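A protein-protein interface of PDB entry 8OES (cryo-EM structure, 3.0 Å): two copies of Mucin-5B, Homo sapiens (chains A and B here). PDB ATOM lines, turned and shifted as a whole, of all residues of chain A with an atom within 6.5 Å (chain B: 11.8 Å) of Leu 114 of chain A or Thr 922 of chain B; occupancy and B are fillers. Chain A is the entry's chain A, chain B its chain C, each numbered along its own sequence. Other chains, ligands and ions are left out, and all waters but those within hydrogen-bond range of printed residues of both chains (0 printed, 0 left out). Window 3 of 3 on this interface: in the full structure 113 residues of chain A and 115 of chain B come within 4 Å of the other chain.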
ATOM      1  N   ILE A 109      19.854  -4.553 -30.350  1.00  0.00           N
ATOM      2  CA  ILE A 109      19.548  -5.629 -29.420  1.00  0.00           C
ATOM      3  C   ILE A 109      19.462  -5.035 -28.028  1.00  0.00           C
ATOM      4  O   ILE A 109      20.440  -4.480 -27.519  1.00  0.00           O
ATOM      5  CB  ILE A 109      20.604  -6.738 -29.465  1.00  0.00           C
ATOM      6  CG1 ILE A 109      20.724  -7.310 -30.871  1.00  0.00           C
ATOM      7  CG2 ILE A 109      20.247  -7.831 -28.490  1.00  0.00           C
ATOM      8  CD1 ILE A 109      21.823  -8.307 -31.003  1.00  0.00           C
ATOM      9  N   LYS A 110      18.298  -5.147 -27.414  1.00  0.00           N
ATOM     10  CA  LYS A 110      18.092  -4.733 -26.037  1.00  0.00           C
ATOM     11  C   LYS A 110      17.878  -5.992 -25.213  1.00  0.00           C
ATOM     12  O   LYS A 110      16.993  -6.795 -25.523  1.00  0.00           O
ATOM     13  CB  LYS A 110      16.896  -3.793 -25.930  1.00  0.00           C
ATOM     14  CG  LYS A 110      16.687  -3.185 -24.567  1.00  0.00           C
ATOM     15  CD  LYS A 110      15.545  -2.193 -24.608  1.00  0.00           C
ATOM     16  CE  LYS A 110      15.322  -1.546 -23.259  1.00  0.00           C
ATOM     17  NZ  LYS A 110      14.231  -0.540 -23.315  1.00  0.00           N
ATOM     18  N   ALA A 111      18.694  -6.175 -24.181  1.00  0.00           N
ATOM     19  CA  ALA A 111      18.628  -7.396 -23.389  1.00  0.00           C
ATOM     20  C   ALA A 111      19.115  -7.120 -21.980  1.00  0.00           C
ATOM     21  O   ALA A 111      20.289  -6.794 -21.781  1.00  0.00           O
ATOM     22  CB  ALA A 111      19.454  -8.509 -24.027  1.00  0.00           C
ATOM     23  N   GLN A 112      18.209  -7.251 -21.015  1.00  0.00           N
ATOM     24  CA  GLN A 112      18.555  -7.259 -19.598  1.00  0.00           C
ATOM     25  C   GLN A 112      19.235  -5.956 -19.191  1.00  0.00           C
ATOM     26  O   GLN A 112      20.166  -5.939 -18.386  1.00  0.00           O
ATOM     27  CB  GLN A 112      19.444  -8.460 -19.274  1.00  0.00           C
ATOM     28  CG  GLN A 112      18.798  -9.829 -19.511  1.00  0.00           C
ATOM     29  CD  GLN A 112      17.626 -10.152 -18.605  1.00  0.00           C
ATOM     30  OE1 GLN A 112      16.878  -9.274 -18.180  1.00  0.00           O
ATOM     31  NE2 GLN A 112      17.444 -11.436 -18.328  1.00  0.00           N
ATOM     32  N   GLY A 113      18.767  -4.850 -19.757  1.00  0.00           N
ATOM     33  CA  GLY A 113      19.352  -3.561 -19.461  1.00  0.00           C
ATOM     34  C   GLY A 113      20.561  -3.196 -20.289  1.00  0.00           C
ATOM     35  O   GLY A 113      21.176  -2.154 -20.034  1.00  0.00           O
ATOM     36  N   LEU A 114      20.922  -4.010 -21.270  1.00  0.00           N
ATOM     37  CA  LEU A 114      22.044  -3.728 -22.148  1.00  0.00           C
ATOM     38  C   LEU A 114      21.515  -3.355 -23.523  1.00  0.00           C
ATOM     39  O   LEU A 114      20.651  -4.047 -24.066  1.00  0.00           O
ATOM     40  CB  LEU A 114      22.976  -4.933 -22.238  1.00  0.00           C
ATOM     41  CG  LEU A 114      24.074  -4.843 -23.290  1.00  0.00           C
ATOM     42  CD1 LEU A 114      25.387  -5.166 -22.641  1.00  0.00           C
ATOM     43  CD2 LEU A 114      23.806  -5.800 -24.434  1.00  0.00           C
ATOM     44  N   VAL A 115      22.027  -2.257 -24.076  1.00  0.00           N
ATOM     45  CA  VAL A 115      21.629  -1.764 -25.389  1.00  0.00           C
ATOM     46  C   VAL A 115      22.816  -1.909 -26.325  1.00  0.00           C
ATOM     47  O   VAL A 115      23.920  -1.451 -26.009  1.00  0.00           O
ATOM     48  CB  VAL A 115      21.157  -0.304 -25.322  1.00  0.00           C
ATOM     49  CG1 VAL A 115      20.709   0.166 -26.685  1.00  0.00           C
ATOM     50  CG2 VAL A 115      20.038  -0.164 -24.320  1.00  0.00           C
ATOM     51  N   LEU A 116      22.591  -2.533 -27.476  1.00  0.00           N
ATOM     52  CA  LEU A 116      23.661  -2.882 -28.402  1.00  0.00           C
ATOM     53  C   LEU A 116      23.231  -2.500 -29.808  1.00  0.00           C
ATOM     54  O   LEU A 116      22.382  -3.168 -30.400  1.00  0.00           O
ATOM     55  CB  LEU A 116      23.963  -4.373 -28.316  1.00  0.00           C
ATOM     56  CG  LEU A 116      25.178  -4.900 -29.057  1.00  0.00           C
ATOM     57  CD1 LEU A 116      25.827  -5.940 -28.190  1.00  0.00           C
ATOM     58  CD2 LEU A 116      24.780  -5.493 -30.394  1.00  0.00           C
ATOM     59  N   ILE A 125      27.822   0.014 -27.424  1.00  0.00           N
ATOM     60  CA  ILE A 125      27.438  -0.739 -26.238  1.00  0.00           C
ATOM     61  C   ILE A 125      26.971   0.262 -25.195  1.00  0.00           C
ATOM     62  O   ILE A 125      27.773   1.044 -24.671  1.00  0.00           O
ATOM     63  CB  ILE A 125      28.592  -1.591 -25.702  1.00  0.00           C
ATOM     64  CG1 ILE A 125      29.222  -2.402 -26.829  1.00  0.00           C
ATOM     65  CG2 ILE A 125      28.092  -2.509 -24.617  1.00  0.00           C
ATOM     66  CD1 ILE A 125      28.290  -3.385 -27.436  1.00  0.00           C
ATOM     67  N   ASN A 126      25.674   0.233 -24.892  1.00  0.00           N
ATOM     68  CA  ASN A 126      25.068   1.158 -23.938  1.00  0.00           C
ATOM     69  C   ASN A 126      25.391   2.605 -24.286  1.00  0.00           C
ATOM     70  O   ASN A 126      25.602   3.440 -23.406  1.00  0.00           O
ATOM     71  CB  ASN A 126      25.495   0.834 -22.508  1.00  0.00           C
ATOM     72  CG  ASN A 126      24.824  -0.411 -21.971  1.00  0.00           C
ATOM     73  OD1 ASN A 126      23.785  -0.832 -22.477  1.00  0.00           O
ATOM     74  ND2 ASN A 126      25.409  -1.003 -20.940  1.00  0.00           N
ATOM     75  N   TYR A 134      34.377  -7.177 -27.149  1.00  0.00           N
ATOM     76  CA  TYR A 134      33.985  -6.555 -25.892  1.00  0.00           C
ATOM     77  C   TYR A 134      33.284  -7.616 -25.065  1.00  0.00           C
ATOM     78  O   TYR A 134      32.281  -8.183 -25.508  1.00  0.00           O
ATOM     79  CB  TYR A 134      33.074  -5.358 -26.149  1.00  0.00           C
ATOM     80  CG  TYR A 134      32.450  -4.731 -24.931  1.00  0.00           C
ATOM     81  CD1 TYR A 134      31.255  -5.210 -24.416  1.00  0.00           C
ATOM     82  CD2 TYR A 134      33.025  -3.629 -24.329  1.00  0.00           C
ATOM     83  CE1 TYR A 134      30.672  -4.630 -23.314  1.00  0.00           C
ATOM     84  CE2 TYR A 134      32.446  -3.037 -23.229  1.00  0.00           C
ATOM     85  CZ  TYR A 134      31.271  -3.542 -22.725  1.00  0.00           C
ATOM     86  OH  TYR A 134      30.694  -2.955 -21.627  1.00  0.00           O
ATOM     87  N   ARG A 136      31.968  -9.111 -21.092  1.00  0.00           N
ATOM     88  CA  ARG A 136      31.520  -8.827 -19.740  1.00  0.00           C
ATOM     89  C   ARG A 136      30.774 -10.053 -19.236  1.00  0.00           C
ATOM     90  O   ARG A 136      30.481 -10.973 -20.001  1.00  0.00           O
ATOM     91  CB  ARG A 136      30.640  -7.576 -19.707  1.00  0.00           C
ATOM     92  CG  ARG A 136      30.708  -6.783 -18.423  1.00  0.00           C
ATOM     93  CD  ARG A 136      32.130  -6.428 -18.051  1.00  0.00           C
ATOM     94  NE  ARG A 136      32.924  -6.015 -19.199  1.00  0.00           N
ATOM     95  CZ  ARG A 136      32.865  -4.817 -19.759  1.00  0.00           C
ATOM     96  NH1 ARG A 136      32.035  -3.889 -19.318  1.00  0.00           N
ATOM     97  NH2 ARG A 136      33.664  -4.541 -20.784  1.00  0.00           N
ATOM     98  N   THR A 137      30.455 -10.056 -17.948  1.00  0.00           N
ATOM     99  CA  THR A 137      29.754 -11.200 -17.378  1.00  0.00           C
ATOM    100  C   THR A 137      28.487 -11.486 -18.164  1.00  0.00           C
ATOM    101  O   THR A 137      27.572 -10.662 -18.201  1.00  0.00           O
ATOM    102  CB  THR A 137      29.418 -10.937 -15.915  1.00  0.00           C
ATOM    103  OG1 THR A 137      28.498  -9.845 -15.833  1.00  0.00           O
ATOM    104  CG2 THR A 137      30.671 -10.588 -15.141  1.00  0.00           C
ATOM    105  N   GLY A 138      28.456 -12.643 -18.824  1.00  0.00           N
ATOM    106  CA  GLY A 138      27.302 -13.084 -19.578  1.00  0.00           C
ATOM    107  C   GLY A 138      27.193 -12.549 -20.989  1.00  0.00           C
ATOM    108  O   GLY A 138      26.358 -13.042 -21.756  1.00  0.00           O
ATOM    109  N   LEU A 139      28.002 -11.565 -21.361  1.00  0.00           N
ATOM    110  CA  LEU A 139      27.942 -10.936 -22.670  1.00  0.00           C
ATOM    111  C   LEU A 139      29.298 -11.024 -23.346  1.00  0.00           C
ATOM    112  O   LEU A 139      30.325 -10.820 -22.700  1.00  0.00           O
ATOM    113  CB  LEU A 139      27.551  -9.469 -22.554  1.00  0.00           C
ATOM    114  CG  LEU A 139      27.772  -8.677 -23.839  1.00  0.00           C
ATOM    115  CD1 LEU A 139      26.630  -8.888 -24.811  1.00  0.00           C
ATOM    116  CD2 LEU A 139      28.022  -7.211 -23.570  1.00  0.00           C
ATOM    117  N   VAL A 150      27.259 -11.543 -31.345  1.00  0.00           N
ATOM    118  CA  VAL A 150      26.932 -11.065 -30.013  1.00  0.00           C
ATOM    119  C   VAL A 150      26.249 -12.211 -29.290  1.00  0.00           C
ATOM    120  O   VAL A 150      25.126 -12.591 -29.636  1.00  0.00           O
ATOM    121  CB  VAL A 150      26.027  -9.832 -30.060  1.00  0.00           C
ATOM    122  CG1 VAL A 150      25.622  -9.431 -28.663  1.00  0.00           C
ATOM    123  CG2 VAL A 150      26.708  -8.694 -30.789  1.00  0.00           C
ATOM    124  N   ILE A 152      24.789 -13.407 -25.729  1.00  0.00           N
ATOM    125  CA  ILE A 152      24.345 -13.054 -24.389  1.00  0.00           C
ATOM    126  C   ILE A 152      23.970 -14.369 -23.724  1.00  0.00           C
ATOM    127  O   ILE A 152      22.877 -14.898 -23.932  1.00  0.00           O
ATOM    128  CB  ILE A 152      23.180 -12.067 -24.422  1.00  0.00           C
ATOM    129  CG1 ILE A 152      23.570 -10.837 -25.239  1.00  0.00           C
ATOM    130  CG2 ILE A 152      22.785 -11.673 -23.022  1.00  0.00           C
ATOM    131  CD1 ILE A 152      22.417  -9.937 -25.571  1.00  0.00           C
ATOM    132  N   ASP B 875      32.703 -13.593  -5.635  1.00  0.00           N
ATOM    133  CA  ASP B 875      33.087 -12.786  -6.784  1.00  0.00           C
ATOM    134  C   ASP B 875      34.316 -13.332  -7.484  1.00  0.00           C
ATOM    135  O   ASP B 875      34.878 -12.660  -8.353  1.00  0.00           O
ATOM    136  CB  ASP B 875      33.336 -11.338  -6.355  1.00  0.00           C
ATOM    137  CG  ASP B 875      33.338 -10.374  -7.525  1.00  0.00           C
ATOM    138  OD1 ASP B 875      32.870 -10.763  -8.614  1.00  0.00           O
ATOM    139  OD2 ASP B 875      33.818  -9.232  -7.363  1.00  0.00           O
ATOM    140  N   GLY B 890      37.008 -13.419 -13.441  1.00  0.00           N
ATOM    141  CA  GLY B 890      36.946 -13.775 -14.842  1.00  0.00           C
ATOM    142  C   GLY B 890      35.520 -13.756 -15.356  1.00  0.00           C
ATOM    143  O   GLY B 890      34.571 -13.944 -14.602  1.00  0.00           O
ATOM    144  N   SER B 891      35.380 -13.526 -16.661  1.00  0.00           N
ATOM    145  CA  SER B 891      34.070 -13.415 -17.280  1.00  0.00           C
ATOM    146  C   SER B 891      33.785 -14.486 -18.317  1.00  0.00           C
ATOM    147  O   SER B 891      32.615 -14.712 -18.633  1.00  0.00           O
ATOM    148  CB  SER B 891      33.915 -12.046 -17.947  1.00  0.00           C
ATOM    149  OG  SER B 891      34.825 -11.921 -19.022  1.00  0.00           O
ATOM    150  N   GLU B 915      31.669 -20.363 -15.468  1.00  0.00           N
ATOM    151  CA  GLU B 915      31.700 -18.971 -15.879  1.00  0.00           C
ATOM    152  C   GLU B 915      30.600 -18.236 -15.139  1.00  0.00           C
ATOM    153  O   GLU B 915      29.641 -18.840 -14.656  1.00  0.00           O
ATOM    154  CB  GLU B 915      31.530 -18.819 -17.385  1.00  0.00           C
ATOM    155  CG  GLU B 915      30.400 -19.633 -17.935  1.00  0.00           C
ATOM    156  CD  GLU B 915      29.273 -18.774 -18.420  1.00  0.00           C
ATOM    157  OE1 GLU B 915      29.383 -17.539 -18.313  1.00  0.00           O
ATOM    158  OE2 GLU B 915      28.277 -19.333 -18.908  1.00  0.00           O
ATOM    159  N   ASN B 916      30.743 -16.921 -15.058  1.00  0.00           N
ATOM    160  CA  ASN B 916      29.905 -16.111 -14.187  1.00  0.00           C
ATOM    161  C   ASN B 916      28.682 -15.617 -14.947  1.00  0.00           C
ATOM    162  O   ASN B 916      28.794 -14.783 -15.850  1.00  0.00           O
ATOM    163  CB  ASN B 916      30.711 -14.948 -13.629  1.00  0.00           C
ATOM    164  CG  ASN B 916      31.679 -15.384 -12.566  1.00  0.00           C
ATOM    165  OD1 ASN B 916      31.541 -16.462 -11.996  1.00  0.00           O
ATOM    166  ND2 ASN B 916      32.670 -14.551 -12.293  1.00  0.00           N
ATOM    167  N   ILE B 917      27.514 -16.124 -14.571  1.00  0.00           N
ATOM    168  CA  ILE B 917      26.248 -15.642 -15.112  1.00  0.00           C
ATOM    169  C   ILE B 917      25.778 -14.440 -14.309  1.00  0.00           C
ATOM    170  O   ILE B 917      25.820 -14.467 -13.073  1.00  0.00           O
ATOM    171  CB  ILE B 917      25.168 -16.729 -15.085  1.00  0.00           C
ATOM    172  CG1 ILE B 917      25.716 -18.030 -15.642  1.00  0.00           C
ATOM    173  CG2 ILE B 917      23.954 -16.280 -15.870  1.00  0.00           C
ATOM    174  CD1 ILE B 917      26.138 -17.907 -17.056  1.00  0.00           C
ATOM    175  N   PRO B 918      25.378 -13.365 -14.947  1.00  0.00           N
ATOM    176  CA  PRO B 918      24.483 -12.423 -14.275  1.00  0.00           C
ATOM    177  C   PRO B 918      23.050 -12.871 -14.488  1.00  0.00           C
ATOM    178  O   PRO B 918      22.688 -13.274 -15.597  1.00  0.00           O
ATOM    179  CB  PRO B 918      24.795 -11.091 -14.959  1.00  0.00           C
ATOM    180  CG  PRO B 918      25.259 -11.481 -16.305  1.00  0.00           C
ATOM    181  CD  PRO B 918      25.958 -12.801 -16.174  1.00  0.00           C
ATOM    182  N   CYS B 919      22.234 -12.836 -13.442  1.00  0.00           N
ATOM    183  CA  CYS B 919      20.909 -13.436 -13.499  1.00  0.00           C
ATOM    184  C   CYS B 919      19.818 -12.477 -13.953  1.00  0.00           C
ATOM    185  O   CYS B 919      18.711 -12.932 -14.262  1.00  0.00           O
ATOM    186  CB  CYS B 919      20.542 -14.017 -12.130  1.00  0.00           C
ATOM    187  SG  CYS B 919      20.483 -12.805 -10.795  1.00  0.00           S
ATOM    188  N   GLY B 920      20.087 -11.178 -14.008  1.00  0.00           N
ATOM    189  CA  GLY B 920      19.063 -10.247 -14.431  1.00  0.00           C
ATOM    190  C   GLY B 920      19.565  -9.094 -15.270  1.00  0.00           C
ATOM    191  O   GLY B 920      18.786  -8.229 -15.674  1.00  0.00           O
ATOM    192  N   THR B 921      20.862  -9.074 -15.549  1.00  0.00           N
ATOM    193  CA  THR B 921      21.473  -7.947 -16.237  1.00  0.00           C
ATOM    194  C   THR B 921      22.748  -8.446 -16.907  1.00  0.00           C
ATOM    195  O   THR B 921      22.926  -9.654 -17.095  1.00  0.00           O
ATOM    196  CB  THR B 921      21.730  -6.789 -15.258  1.00  0.00           C
ATOM    197  OG1 THR B 921      22.178  -5.637 -15.981  1.00  0.00           O
ATOM    198  CG2 THR B 921      22.779  -7.179 -14.226  1.00  0.00           C
ATOM    199  N   THR B 922      23.613  -7.516 -17.309  1.00  0.00           N
ATOM    200  CA  THR B 922      24.982  -7.831 -17.712  1.00  0.00           C
ATOM    201  C   THR B 922      25.878  -6.913 -16.891  1.00  0.00           C
ATOM    202  O   THR B 922      26.323  -5.864 -17.361  1.00  0.00           O
ATOM    203  CB  THR B 922      25.168  -7.643 -19.198  1.00  0.00           C
ATOM    204  OG1 THR B 922      24.699  -6.342 -19.569  1.00  0.00           O
ATOM    205  CG2 THR B 922      24.365  -8.687 -19.949  1.00  0.00           C
ATOM    206  N   GLY B 923      26.138  -7.322 -15.655  1.00  0.00           N
ATOM    207  CA  GLY B 923      26.884  -6.515 -14.712  1.00  0.00           C
ATOM    208  C   GLY B 923      27.698  -7.362 -13.762  1.00  0.00           C
ATOM    209  O   GLY B 923      28.446  -8.245 -14.188  1.00  0.00           O
ATOM    210  N   THR B 924      27.567  -7.090 -12.468  1.00  0.00           N
ATOM    211  CA  THR B 924      28.202  -7.927 -11.462  1.00  0.00           C
ATOM    212  C   THR B 924      27.567  -9.313 -11.463  1.00  0.00           C
ATOM    213  O   THR B 924      26.374  -9.468 -11.736  1.00  0.00           O
ATOM    214  CB  THR B 924      28.081  -7.286 -10.082  1.00  0.00           C
ATOM    215  OG1 THR B 924      28.264  -5.871 -10.199  1.00  0.00           O
ATOM    216  CG2 THR B 924      29.140  -7.844  -9.143  1.00  0.00           C
ATOM    217  N   THR B 925      28.380 -10.322 -11.159  1.00  0.00           N
ATOM    218  CA  THR B 925      27.944 -11.706 -11.270  1.00  0.00           C
ATOM    219  C   THR B 925      26.834 -11.994 -10.272  1.00  0.00           C
ATOM    220  O   THR B 925      26.809 -11.440  -9.171  1.00  0.00           O
ATOM    221  CB  THR B 925      29.121 -12.636 -11.013  1.00  0.00           C
ATOM    222  OG1 THR B 925      29.423 -12.633  -9.618  1.00  0.00           O
ATOM    223  CG2 THR B 925      30.333 -12.109 -11.732  1.00  0.00           C
ATOM    224  N   CYS B 926      25.903 -12.864 -10.661  1.00  0.00           N
ATOM    225  CA  CYS B 926      24.813 -13.266  -9.793  1.00  0.00           C
ATOM    226  C   CYS B 926      24.736 -14.766  -9.601  1.00  0.00           C
ATOM    227  O   CYS B 926      24.214 -15.213  -8.576  1.00  0.00           O
ATOM    228  CB  CYS B 926      23.475 -12.758 -10.353  1.00  0.00           C
ATOM    229  SG  CYS B 926      21.985 -13.380  -9.553  1.00  0.00           S
ATOM    230  N   SER B 927      25.255 -15.550 -10.537  1.00  0.00           N
ATOM    231  CA  SER B 927      25.269 -16.998 -10.409  1.00  0.00           C
ATOM    232  C   SER B 927      26.363 -17.546 -11.316  1.00  0.00           C
ATOM    233  O   SER B 927      27.146 -16.796 -11.900  1.00  0.00           O
ATOM    234  CB  SER B 927      23.902 -17.594 -10.745  1.00  0.00           C
ATOM    235  OG  SER B 927      23.731 -18.849 -10.112  1.00  0.00           O
ATOM    236  N   ALA B1090      31.302  -5.197  -3.260  1.00  0.00           N
ATOM    237  CA  ALA B1090      31.259  -5.221  -4.716  1.00  0.00           C
ATOM    238  C   ALA B1090      29.837  -5.196  -5.257  1.00  0.00           C
ATOM    239  O   ALA B1090      29.573  -4.551  -6.276  1.00  0.00           O
ATOM    240  CB  ALA B1090      31.995  -6.453  -5.238  1.00  0.00           C
ATOM    241  N   ASP B1092      27.154  -3.811  -5.935  1.00  0.00           N
ATOM    242  CA  ASP B1092      26.474  -2.524  -5.945  1.00  0.00           C
ATOM    243  C   ASP B1092      25.379  -2.434  -6.991  1.00  0.00           C
ATOM    244  O   ASP B1092      24.794  -1.360  -7.158  1.00  0.00           O
ATOM    245  CB  ASP B1092      27.469  -1.393  -6.190  1.00  0.00           C
ATOM    246  CG  ASP B1092      28.240  -1.576  -7.466  1.00  0.00           C
ATOM    247  OD1 ASP B1092      28.212  -2.697  -8.011  1.00  0.00           O
ATOM    248  OD2 ASP B1092      28.859  -0.600  -7.934  1.00  0.00           O
ATOM    249  N   SER B1093      25.100  -3.514  -7.713  1.00  0.00           N
ATOM    250  CA  SER B1093      24.075  -3.472  -8.740  1.00  0.00           C
ATOM    251  C   SER B1093      22.828  -4.258  -8.379  1.00  0.00           C
ATOM    252  O   SER B1093      21.889  -4.294  -9.177  1.00  0.00           O
ATOM    253  CB  SER B1093      24.625  -3.996 -10.062  1.00  0.00           C
ATOM    254  OG  SER B1093      23.636  -3.910 -11.068  1.00  0.00           O
ATOM    255  N   GLY B1094      22.796  -4.893  -7.224  1.00  0.00           N
ATOM    256  CA  GLY B1094      21.616  -5.605  -6.773  1.00  0.00           C
ATOM    257  C   GLY B1094      21.961  -6.987  -6.262  1.00  0.00           C
ATOM    258  O   GLY B1094      22.967  -7.589  -6.628  1.00  0.00           O
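Gln 112 of chain A touches Thr 922 of chain B (O to N, 3.9 Å). Leu 114 of chain A touches Thr 922 of chain B. Arg 136 of chain A touches Ser 891 of chain B. Ser 891 of chain B touches Thr 137 of chain A. Asn 916 of chain B touches Thr 137 of chain A (O to CB, 3.9 Å). Thr 137 of chain A touches Pro 918 of chain B. CA of Thr 922 of chain B touches O of Thr 137 of chain A (3.9 Å). Thr 137 of chain A touches Thr 925 of chain B. Gly 138 of chain A touches Asn 916 of chain B (N to O, 3.7 Å). Pro 918 of chain B touches Gly 138 of chain A.
The side-chain hydroxyl of Tyr 134 of chain A sits at hydrogen-bond distance from the guanidinium group of Arg 136 of chain A, at 2.8 Å. The side-chain amide nitrogen (ND2) of Asn 916 of chain B lies within hydrogen-bond range of the backbone carbonyl oxygen (O) of Gly 890 of chain B (3.1 Å). The side-chain sulfur (SG) of Cys 919 of chain B forms a disulfide with the side-chain sulfur (SG) of Cys 926 of chain B (2.0 Å).
The backbone carbonyl oxygen of Gly 920 of chain B sits close to the side-chain amide oxygen of Gln 112 of chain A. OG1 of Thr 921 of chain B sits at hydrogen-bond distance from O of Gln 112 of chain A (3.2 Å). The backbone NH (N) of Gly 923 of chain B lies close to the side-chain hydroxyl (OG1) of Thr 137 of chain A (3.5 Å).
No position is printed for both chains. Of the 13 pairs that touch across the chains among the printed residues, none has its exchanged pair printed and touching as well.
No residue of chain B comes within 4 Å of Ile 109 of chain A. No residue of chain B comes within 4 Å of Lys 110 of chain A. Ala 111 of chain A touches none of the printed residues of chain B. Gln 112 of chain A touches just these residues of chain B: Gly 920 (3.3 Å), Thr 921 (3.2 Å) and Thr 922 (3.9 Å). No residue of chain B comes within 4 Å of Gly 113 of chain A. Leu 114 of chain A touches one residue of chain B. Val 115 of chain A touches none of the printed residues of chain B. No residue of chain B comes within 4 Å of Leu 116 of chain A. No residue of chain B comes within 4 Å of Ile 125 of chain A. Tyr 134 of chain A touches none of the printed residues of chain B. Of the printed residues of chain B, Thr 137 of chain A touches Ser 891, Asn 916, Pro 918, Thr 922, Gly 923 and Thr 925. Gly 138 of chain A touches two residues of chain B. No residue of chain B comes within 4 Å of Leu 139 of chain A. No residue of chain B comes within 4 Å of Ile 152 of chain A. Of the printed residues of chain A, Gly 920 of chain B touches Gln 112 (3.3 Å). The nearest printed residue of chain A that does not touch Thr 922 of chain B is Leu 139 of chain A (4.2 Å).
Of the 17 printed residues of chain A, 5 touch a printed residue of chain B. Of the 20 printed residues of chain B, 8 touch a printed residue of chain A. Printed residues of chain B that touch a printed residue of chain A: Ser 891, Asn 916, Pro 918, Gly 920, Thr 921, Thr 922, Gly 923 and Thr 925. Hydrophobic or aromatic side chains of chain B that line the printed part of chain A: Pro 918. Among the printed residues, 13 pairs touch across the chains. Among the printed residues, no Asp or Glu carboxylate lies within 4 Å of a Lys or Arg side-chain nitrogen of the other chain.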
